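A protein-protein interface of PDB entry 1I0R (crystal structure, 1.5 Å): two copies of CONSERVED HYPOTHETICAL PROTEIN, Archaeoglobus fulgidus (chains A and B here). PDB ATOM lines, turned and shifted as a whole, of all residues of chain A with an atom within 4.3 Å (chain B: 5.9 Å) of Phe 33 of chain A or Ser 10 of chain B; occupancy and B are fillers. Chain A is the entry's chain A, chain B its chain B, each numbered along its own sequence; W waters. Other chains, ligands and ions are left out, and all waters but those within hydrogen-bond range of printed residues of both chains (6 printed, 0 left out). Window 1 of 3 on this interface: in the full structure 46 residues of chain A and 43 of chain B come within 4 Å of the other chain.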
ATOM      1  N   SER A  10      22.032 -19.853  13.122  1.00  0.00           N
ATOM      2  CA  SER A  10      22.934 -18.700  13.307  1.00  0.00           C
ATOM      3  C   SER A  10      23.587 -18.624  14.666  1.00  0.00           C
ATOM      4  O   SER A  10      22.995 -18.986  15.689  1.00  0.00           O
ATOM      5  CB  SER A  10      22.202 -17.380  13.095  1.00  0.00           C
ATOM      6  OG  SER A  10      21.776 -17.260  11.751  1.00  0.00           O
ATOM      7  N   TYR A  11      24.828 -18.134  14.679  1.00  0.00           N
ATOM      8  CA  TYR A  11      25.555 -17.986  15.964  1.00  0.00           C
ATOM      9  C   TYR A  11      26.503 -16.809  15.895  1.00  0.00           C
ATOM     10  O   TYR A  11      26.793 -16.300  14.813  1.00  0.00           O
ATOM     11  CB  TYR A  11      26.489 -19.182  16.247  1.00  0.00           C
ATOM     12  CG  TYR A  11      25.913 -20.595  16.201  1.00  0.00           C
ATOM     13  CD1 TYR A  11      25.629 -21.220  14.988  1.00  0.00           C
ATOM     14  CD2 TYR A  11      25.646 -21.289  17.384  1.00  0.00           C
ATOM     15  CE1 TYR A  11      25.086 -22.498  14.961  1.00  0.00           C
ATOM     16  CE2 TYR A  11      25.105 -22.557  17.362  1.00  0.00           C
ATOM     17  CZ  TYR A  11      24.826 -23.157  16.151  1.00  0.00           C
ATOM     18  OH  TYR A  11      24.267 -24.409  16.153  1.00  0.00           O
ATOM     19  N   GLY A  12      26.985 -16.376  17.066  1.00  0.00           N
ATOM     20  CA  GLY A  12      28.060 -15.379  17.121  1.00  0.00           C
ATOM     21  C   GLY A  12      29.359 -16.186  17.253  1.00  0.00           C
ATOM     22  O   GLY A  12      29.399 -17.400  17.055  1.00  0.00           O
ATOM     23  N   TYR A  14      32.813 -16.303  19.935  1.00  0.00           N
ATOM     24  CA  TYR A  14      33.247 -15.803  21.246  1.00  0.00           C
ATOM     25  C   TYR A  14      34.452 -16.511  21.789  1.00  0.00           C
ATOM     26  O   TYR A  14      34.828 -17.587  21.312  1.00  0.00           O
ATOM     27  CB  TYR A  14      32.106 -16.118  22.250  1.00  0.00           C
ATOM     28  CG  TYR A  14      30.696 -15.789  21.793  1.00  0.00           C
ATOM     29  CD1 TYR A  14      29.932 -16.704  21.027  1.00  0.00           C
ATOM     30  CD2 TYR A  14      30.160 -14.539  22.057  1.00  0.00           C
ATOM     31  CE1 TYR A  14      28.653 -16.349  20.537  1.00  0.00           C
ATOM     32  CE2 TYR A  14      28.902 -14.167  21.576  1.00  0.00           C
ATOM     33  CZ  TYR A  14      28.155 -15.074  20.819  1.00  0.00           C
ATOM     34  OH  TYR A  14      26.907 -14.686  20.344  1.00  0.00           O
ATOM     35  N   ASN A  30      31.016 -21.034  19.615  1.00  0.00           N
ATOM     36  CA  ASN A  30      29.940 -20.327  18.934  1.00  0.00           C
ATOM     37  C   ASN A  30      28.633 -20.559  19.708  1.00  0.00           C
ATOM     38  O   ASN A  30      27.680 -19.816  19.545  1.00  0.00           O
ATOM     39  CB  ASN A  30      29.795 -20.750  17.435  1.00  0.00           C
ATOM     40  CG  ASN A  30      29.472 -22.217  17.232  1.00  0.00           C
ATOM     41  OD1 ASN A  30      29.948 -23.089  17.936  1.00  0.00           O
ATOM     42  ND2 ASN A  30      28.665 -22.501  16.197  1.00  0.00           N
ATOM     43  N   THR A  31      28.609 -21.552  20.587  1.00  0.00           N
ATOM     44  CA  THR A  31      27.370 -21.892  21.297  1.00  0.00           C
ATOM     45  C   THR A  31      27.232 -21.144  22.610  1.00  0.00           C
ATOM     46  O   THR A  31      27.508 -21.700  23.669  1.00  0.00           O
ATOM     47  CB  THR A  31      27.337 -23.410  21.543  1.00  0.00           C
ATOM     48  OG1 THR A  31      27.744 -24.108  20.347  1.00  0.00           O
ATOM     49  CG2 THR A  31      25.965 -23.848  21.904  1.00  0.00           C
ATOM     50  N   VAL A  32      26.860 -19.870  22.508  1.00  0.00           N
ATOM     51  CA  VAL A  32      26.709 -18.958  23.654  1.00  0.00           C
ATOM     52  C   VAL A  32      25.415 -18.188  23.422  1.00  0.00           C
ATOM     53  O   VAL A  32      25.242 -17.593  22.356  1.00  0.00           O
ATOM     54  CB  VAL A  32      27.883 -17.922  23.707  1.00  0.00           C
ATOM     55  CG1 VAL A  32      27.673 -16.903  24.807  1.00  0.00           C
ATOM     56  CG2 VAL A  32      29.207 -18.669  23.888  1.00  0.00           C
ATOM     57  N   PHE A  33      24.519 -18.183  24.399  1.00  0.00           N
ATOM     58  CA  PHE A  33      23.231 -17.494  24.212  1.00  0.00           C
ATOM     59  C   PHE A  33      22.610 -17.069  25.533  1.00  0.00           C
ATOM     60  O   PHE A  33      22.807 -17.719  26.561  1.00  0.00           O
ATOM     61  CB  PHE A  33      22.195 -18.442  23.565  1.00  0.00           C
ATOM     62  CG  PHE A  33      22.539 -18.896  22.176  1.00  0.00           C
ATOM     63  CD1 PHE A  33      23.414 -19.955  21.957  1.00  0.00           C
ATOM     64  CD2 PHE A  33      22.000 -18.232  21.071  1.00  0.00           C
ATOM     65  CE1 PHE A  33      23.763 -20.356  20.640  1.00  0.00           C
ATOM     66  CE2 PHE A  33      22.328 -18.613  19.769  1.00  0.00           C
ATOM     67  CZ  PHE A  33      23.215 -19.679  19.550  1.00  0.00           C
ATOM     68  N   GLN A  34      21.853 -15.979  25.504  1.00  0.00           N
ATOM     69  CA  GLN A  34      21.143 -15.556  26.713  1.00  0.00           C
ATOM     70  C   GLN A  34      19.877 -16.427  26.818  1.00  0.00           C
ATOM     71  O   GLN A  34      19.192 -16.656  25.820  1.00  0.00           O
ATOM     72  CB  GLN A  34      20.729 -14.097  26.603  1.00  0.00           C
ATOM     73  CG  GLN A  34      19.940 -13.633  27.828  1.00  0.00           C
ATOM     74  CD  GLN A  34      19.723 -12.118  27.862  1.00  0.00           C
ATOM     75  OE1 GLN A  34      20.133 -11.374  26.962  1.00  0.00           O
ATOM     76  NE2 GLN A  34      19.070 -11.650  28.927  1.00  0.00           N
ATOM     77  N   LEU A  35      19.580 -16.919  28.014  1.00  0.00           N
ATOM     78  CA  LEU A  35      18.386 -17.752  28.199  1.00  0.00           C
ATOM     79  C   LEU A  35      17.228 -17.015  28.822  1.00  0.00           C
ATOM     80  O   LEU A  35      16.074 -17.228  28.430  1.00  0.00           O
ATOM     81  CB  LEU A  35      18.691 -18.966  29.080  1.00  0.00           C
ATOM     82  CG  LEU A  35      19.706 -19.950  28.502  1.00  0.00           C
ATOM     83  CD1 LEU A  35      19.634 -21.276  29.190  1.00  0.00           C
ATOM     84  CD2 LEU A  35      19.367 -20.163  27.052  1.00  0.00           C
ATOM     85  N   ILE A  42      23.086 -16.556  31.103  1.00  0.00           N
ATOM     86  CA  ILE A  42      23.745 -16.861  29.830  1.00  0.00           C
ATOM     87  C   ILE A  42      24.186 -18.324  29.832  1.00  0.00           C
ATOM     88  O   ILE A  42      24.722 -18.844  30.812  1.00  0.00           O
ATOM     89  CB  ILE A  42      25.052 -16.020  29.665  1.00  0.00           C
ATOM     90  CG1 ILE A  42      24.780 -14.529  29.847  1.00  0.00           C
ATOM     91  CG2 ILE A  42      25.690 -16.266  28.287  1.00  0.00           C
ATOM     92  CD1 ILE A  42      23.844 -13.927  28.848  1.00  0.00           C
ATOM     93  N   ALA A  43      24.007 -19.009  28.718  1.00  0.00           N
ATOM     94  CA  ALA A  43      24.446 -20.395  28.616  1.00  0.00           C
ATOM     95  C   ALA A  43      25.639 -20.532  27.666  1.00  0.00           C
ATOM     96  O   ALA A  43      25.736 -19.782  26.673  1.00  0.00           O
ATOM     97  CB  ALA A  43      23.311 -21.284  28.081  1.00  0.00           C
ATOM     98  N   VAL A 144      30.183  -7.075  15.280  1.00  0.00           N
ATOM     99  CA  VAL A 144      30.561  -8.366  15.830  1.00  0.00           C
ATOM    100  C   VAL A 144      30.817  -9.349  14.703  1.00  0.00           C
ATOM    101  O   VAL A 144      30.378  -9.152  13.567  1.00  0.00           O
ATOM    102  CB  VAL A 144      29.451  -8.964  16.754  1.00  0.00           C
ATOM    103  CG1 VAL A 144      29.115  -7.979  17.874  1.00  0.00           C
ATOM    104  CG2 VAL A 144      28.205  -9.342  15.942  1.00  0.00           C
ATOM    105  N   THR A 146      30.144 -12.914  13.142  1.00  0.00           N
ATOM    106  CA  THR A 146      29.192 -14.012  13.275  1.00  0.00           C
ATOM    107  C   THR A 146      29.860 -15.310  12.840  1.00  0.00           C
ATOM    108  O   THR A 146      30.917 -15.306  12.194  1.00  0.00           O
ATOM    109  CB  THR A 146      27.924 -13.783  12.429  1.00  0.00           C
ATOM    110  OG1 THR A 146      28.256 -13.835  11.031  1.00  0.00           O
ATOM    111  CG2 THR A 146      27.311 -12.446  12.744  1.00  0.00           C
ATOM    112  N   TYR B   7      23.134  -7.407  24.021  1.00  0.00           N
ATOM    113  CA  TYR B   7      22.611  -7.230  22.684  1.00  0.00           C
ATOM    114  C   TYR B   7      23.668  -7.496  21.615  1.00  0.00           C
ATOM    115  O   TYR B   7      23.372  -7.437  20.419  1.00  0.00           O
ATOM    116  CB  TYR B   7      22.031  -5.820  22.532  1.00  0.00           C
ATOM    117  CG  TYR B   7      20.734  -5.631  23.293  1.00  0.00           C
ATOM    118  CD1 TYR B   7      19.504  -5.889  22.685  1.00  0.00           C
ATOM    119  CD2 TYR B   7      20.735  -5.217  24.627  1.00  0.00           C
ATOM    120  CE1 TYR B   7      18.289  -5.729  23.395  1.00  0.00           C
ATOM    121  CE2 TYR B   7      19.521  -5.056  25.351  1.00  0.00           C
ATOM    122  CZ  TYR B   7      18.311  -5.310  24.717  1.00  0.00           C
ATOM    123  OH  TYR B   7      17.106  -5.120  25.381  1.00  0.00           O
ATOM    124  N   LYS B   8      24.900  -7.782  22.053  1.00  0.00           N
ATOM    125  CA  LYS B   8      25.989  -8.084  21.132  1.00  0.00           C
ATOM    126  C   LYS B   8      26.019  -9.582  20.812  1.00  0.00           C
ATOM    127  O   LYS B   8      26.770 -10.015  19.945  1.00  0.00           O
ATOM    128  CB  LYS B   8      27.340  -7.639  21.714  1.00  0.00           C
ATOM    129  CG  LYS B   8      27.431  -6.131  22.012  1.00  0.00           C
ATOM    130  CD  LYS B   8      27.193  -5.301  20.758  1.00  0.00           C
ATOM    131  CE  LYS B   8      27.482  -3.842  21.064  1.00  0.00           C
ATOM    132  NZ  LYS B   8      27.134  -2.981  19.904  1.00  0.00           N
ATOM    133  N   ILE B   9      25.220 -10.370  21.533  1.00  0.00           N
ATOM    134  CA  ILE B   9      25.125 -11.815  21.285  1.00  0.00           C
ATOM    135  C   ILE B   9      24.260 -12.026  20.023  1.00  0.00           C
ATOM    136  O   ILE B   9      23.202 -11.393  19.860  1.00  0.00           O
ATOM    137  CB  ILE B   9      24.484 -12.532  22.497  1.00  0.00           C
ATOM    138  CG1 ILE B   9      25.398 -12.368  23.713  1.00  0.00           C
ATOM    139  CG2 ILE B   9      24.213 -14.006  22.178  1.00  0.00           C
ATOM    140  CD1 ILE B   9      24.785 -12.917  25.007  1.00  0.00           C
ATOM    141  N   SER B  10      24.704 -12.920  19.140  1.00  0.00           N
ATOM    142  CA  SER B  10      24.013 -13.172  17.861  1.00  0.00           C
ATOM    143  C   SER B  10      23.024 -14.355  17.876  1.00  0.00           C
ATOM    144  O   SER B  10      23.262 -15.387  18.502  1.00  0.00           O
ATOM    145  CB  SER B  10      25.057 -13.409  16.744  1.00  0.00           C
ATOM    146  OG  SER B  10      25.849 -12.236  16.513  1.00  0.00           O
ATOM    147  N   TYR B  11      21.899 -14.191  17.168  1.00  0.00           N
ATOM    148  CA  TYR B  11      20.875 -15.233  17.078  1.00  0.00           C
ATOM    149  C   TYR B  11      20.261 -15.298  15.687  1.00  0.00           C
ATOM    150  O   TYR B  11      20.398 -14.373  14.881  1.00  0.00           O
ATOM    151  CB  TYR B  11      19.688 -14.949  18.012  1.00  0.00           C
ATOM    152  CG  TYR B  11      19.990 -14.706  19.469  1.00  0.00           C
ATOM    153  CD1 TYR B  11      20.459 -13.467  19.911  1.00  0.00           C
ATOM    154  CD2 TYR B  11      19.808 -15.721  20.405  1.00  0.00           C
ATOM    155  CE1 TYR B  11      20.751 -13.249  21.255  1.00  0.00           C
ATOM    156  CE2 TYR B  11      20.084 -15.525  21.744  1.00  0.00           C
ATOM    157  CZ  TYR B  11      20.567 -14.290  22.173  1.00  0.00           C
ATOM    158  OH  TYR B  11      20.942 -14.088  23.472  1.00  0.00           O
ATOM    159  N   GLY B  12      19.580 -16.411  15.429  1.00  0.00           N
ATOM    160  CA  GLY B  12      18.841 -16.536  14.176  1.00  0.00           C
ATOM    161  C   GLY B  12      17.384 -16.180  14.511  1.00  0.00           C
ATOM    162  O   GLY B  12      17.095 -15.648  15.577  1.00  0.00           O
ATOM    163  N   ASN B  30      14.158 -16.862  19.017  1.00  0.00           N
ATOM    164  CA  ASN B  30      15.493 -16.576  18.493  1.00  0.00           C
ATOM    165  C   ASN B  30      16.515 -17.499  19.180  1.00  0.00           C
ATOM    166  O   ASN B  30      17.643 -17.656  18.698  1.00  0.00           O
ATOM    167  CB  ASN B  30      15.859 -15.077  18.674  1.00  0.00           C
ATOM    168  CG  ASN B  30      16.086 -14.678  20.126  1.00  0.00           C
ATOM    169  OD1 ASN B  30      15.620 -15.334  21.051  1.00  0.00           O
ATOM    170  ND2 ASN B  30      16.808 -13.573  20.325  1.00  0.00           N
ATOM    171  N   THR B  31      16.096 -18.195  20.238  1.00  0.00           N
ATOM    172  CA  THR B  31      17.042 -19.020  20.993  1.00  0.00           C
ATOM    173  C   THR B  31      16.971 -20.502  20.657  1.00  0.00           C
ATOM    174  O   THR B  31      16.327 -21.305  21.358  1.00  0.00           O
ATOM    175  CB  THR B  31      16.857 -18.756  22.507  1.00  0.00           C
ATOM    176  OG1 THR B  31      17.006 -17.343  22.745  1.00  0.00           O
ATOM    177  CG2 THR B  31      17.917 -19.486  23.334  1.00  0.00           C
ATOM    178  N   VAL B  32      17.630 -20.842  19.549  1.00  0.00           N
ATOM    179  CA  VAL B  32      17.703 -22.197  19.015  1.00  0.00           C
ATOM    180  C   VAL B  32      19.159 -22.406  18.639  1.00  0.00           C
ATOM    181  O   VAL B  32      19.754 -21.582  17.932  1.00  0.00           O
ATOM    182  CB  VAL B  32      16.850 -22.352  17.743  1.00  0.00           C
ATOM    183  CG1 VAL B  32      17.072 -23.719  17.125  1.00  0.00           C
ATOM    184  CG2 VAL B  32      15.361 -22.111  18.087  1.00  0.00           C
ATOM    185  N   PHE B  33      19.733 -23.492  19.128  1.00  0.00           N
ATOM    186  CA  PHE B  33      21.135 -23.763  18.865  1.00  0.00           C
ATOM    187  C   PHE B  33      21.469 -25.236  18.942  1.00  0.00           C
ATOM    188  O   PHE B  33      20.874 -25.986  19.705  1.00  0.00           O
ATOM    189  CB  PHE B  33      22.031 -22.923  19.803  1.00  0.00           C
ATOM    190  CG  PHE B  33      21.717 -23.040  21.279  1.00  0.00           C
ATOM    191  CD1 PHE B  33      22.510 -23.820  22.101  1.00  0.00           C
ATOM    192  CD2 PHE B  33      20.726 -22.258  21.865  1.00  0.00           C
ATOM    193  CE1 PHE B  33      22.329 -23.814  23.506  1.00  0.00           C
ATOM    194  CE2 PHE B  33      20.535 -22.246  23.254  1.00  0.00           C
ATOM    195  CZ  PHE B  33      21.343 -23.025  24.074  1.00  0.00           C
ATOM    196  N   TYR B 147      18.462 -12.464  13.875  1.00  0.00           N
ATOM    197  CA  TYR B 147      17.687 -11.653  14.809  1.00  0.00           C
ATOM    198  C   TYR B 147      18.037 -10.171  14.669  1.00  0.00           C
ATOM    199  O   TYR B 147      17.153  -9.312  14.717  1.00  0.00           O
ATOM    200  CB  TYR B 147      17.940 -12.131  16.247  1.00  0.00           C
ATOM    201  CG  TYR B 147      17.231 -11.337  17.319  1.00  0.00           C
ATOM    202  CD1 TYR B 147      15.845 -11.371  17.434  1.00  0.00           C
ATOM    203  CD2 TYR B 147      17.949 -10.577  18.243  1.00  0.00           C
ATOM    204  CE1 TYR B 147      15.186 -10.668  18.452  1.00  0.00           C
ATOM    205  CE2 TYR B 147      17.302  -9.867  19.265  1.00  0.00           C
ATOM    206  CZ  TYR B 147      15.923  -9.924  19.361  1.00  0.00           C
ATOM    207  OH  TYR B 147      15.278  -9.264  20.393  1.00  0.00           O
HETATM  208  O   HOH W   1      15.697 -17.614  25.597  1.00  0.00           O
HETATM  209  O   HOH W   2      25.352 -16.749  19.599  1.00  0.00           O
HETATM  210  O   HOH W   3      27.671 -12.126  18.403  1.00  0.00           O
HETATM  211  O   HOH W   4      21.163 -11.541  24.336  1.00  0.00           O
HETATM  212  O   HOH W   5      20.481 -19.170  16.677  1.00  0.00           O
HETATM  213  O   HOH W   6      17.420 -14.464  24.295  1.00  0.00           O
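N of Gln 34 of chain A lies within hydrogen-bond range of OH of Tyr 11 of chain B (2.9 Å).
OH of Tyr 14 of chain A is in hydrogen-bond range of N of Ser 10 of chain B (3.1 Å).
O of Tyr 11 of chain B lies within hydrogen-bond range of N of Tyr 147 of chain B (2.9 Å).
The backbone carbonyl oxygen of Phe 33 of chain A sits at hydrogen-bond distance from the backbone NH of Ala 43 of chain A, 2.8 Å away.
The side-chain amide oxygen (OD1) of Asn 30 of chain A lies within hydrogen-bond range of the side-chain hydroxyl (OG1) of Thr 31 of chain A, at 3.4 Å.
OG1 of Thr 31 of chain B sits at hydrogen-bond distance from OD1 of Asn 30 of chain B (3.0 Å).
Among the printed residues, pairs that only touch across the chains: Ser 10 of chain A with Tyr 11 of chain B (3.8 Å), Ser 10 of chain A with Gly 12 of chain B (3.6 Å), Tyr 11 of chain A with Ser 10 of chain B (3.8 Å), Tyr 11 of chain A with Phe 33 of chain B (3.9 Å), Gly 12 of chain A with Ser 10 of chain B (3.6 Å), Tyr 14 of chain A with Ile 9 of chain B (3.3 Å), Thr 31 of chain A with Phe 33 of chain B (3.5 Å), Val 32 of chain A with Ile 9 of chain B (3.7 Å), Phe 33 of chain A with Ser 10 of chain B (3.6 Å), Phe 33 of chain A with Tyr 11 of chain B (3.4 Å), Phe 33 of chain A with Phe 33 of chain B (3.2 Å), Gln 34 of chain A with Thr 31 of chain B (3.8 Å), Val 144 of chain A with Lys 8 of chain B (3.7 Å) and Val 144 of chain A with Ser 10 of chain B (3.8 Å).
Of the printed residues of chain B, Phe 33 of chain A touches Ser 10 (3.6 Å), Tyr 11 (3.4 Å) and Phe 33 (3.2 Å).
Of the printed residues of chain A, Ser 10 of chain B touches Tyr 11 (3.8 Å), Gly 12 (3.6 Å), Tyr 14 (3.1 Å), Phe 33 (3.6 Å) and Val 144 (3.8 Å).
Of the printed residues of chain A, Lys 8 of chain B touches Val 144 (3.7 Å).
Printed residues of chain B within 4 Å of Ser 10 of chain A: Tyr 11 (3.8 Å) and Gly 12 (3.6 Å).
Printed residues of chain B within 4 Å of Gln 34 of chain A: Tyr 11 and Thr 31.
Leu 35 of chain A touches none of the printed residues of chain B.
Asn 30 of chain B touches none of the printed residues of chain A.
The nearest printed residue of chain A that does not touch Ser 10 of chain B is Thr 146 of chain A (4.05 Å).
Of the 14 printed residues of chain A, 9 touch a printed residue of chain B.
Printed residues of chain B that touch a printed residue of chain A: Lys 8, Ile 9, Ser 10, Tyr 11, Gly 12, Thr 31 and Phe 33.
Among the printed residues, 16 pairs touch across the chains.
Among the printed residues, no Asp or Glu carboxylate lies within 4 Å of a Lys or Arg side-chain nitrogen of the other chain.
Ser 10 of chain A touches Tyr 11 of chain B, and with the chains exchanged Tyr 11 of chain A touches Ser 10 of chain B.
Tyr 11 of chain A touches Phe 33 of chain B, and with the chains exchanged Phe 33 of chain A touches Tyr 11 of chain B.
Thr 31 of chain A touches Phe 33 of chain B, but with the chains exchanged Phe 33 of chain A does not touch Thr 31 of chain B (4.4 Å).
Phe 33 of chain B touches its own counterpart, Phe 33 of chain A.
Of the 16 pairs that touch across the chains among the printed residues, 7 have their exchanged pair printed and touching as well.
Water W3 lies within hydrogen-bond range of the side-chain hydroxyl of Ser 10 of chain B, the backbone carbonyl oxygen of Lys 8 of chain B and the side-chain hydroxyl of Tyr 14 of chain A.
Water W2 lies within hydrogen-bond range of the side-chain hydroxyl of Tyr 14 of chain A (2.7 Å), the backbone carbonyl oxygen of Ser 10 of chain B (2.7 Å), the backbone carbonyl oxygen of Val 32 of chain A (2.9 Å) and the backbone NH of Gly 12 of chain A (3.0 Å).
Water W4 bridges OH of Tyr 11 of chain B (2.7 Å) and OE1 of Gln 34 of chain A (2.8 Å).
Water W5 lies within hydrogen-bond range of the backbone carbonyl oxygen of Ser 10 of chain A (2.7 Å), the backbone carbonyl oxygen of Val 32 of chain B (2.8 Å) and the backbone NH of Gly 12 of chain B (3.2 Å).
Water W1 bridges the backbone carbonyl oxygen of Leu 35 of chain A (2.9 Å) and the side-chain hydroxyl of Thr 31 of chain B (3.1 Å).
Water W6 bridges the backbone carbonyl oxygen of Gln 34 of chain A (3.2 Å) and the side-chain hydroxyl of Thr 31 of chain B (3.3 Å).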
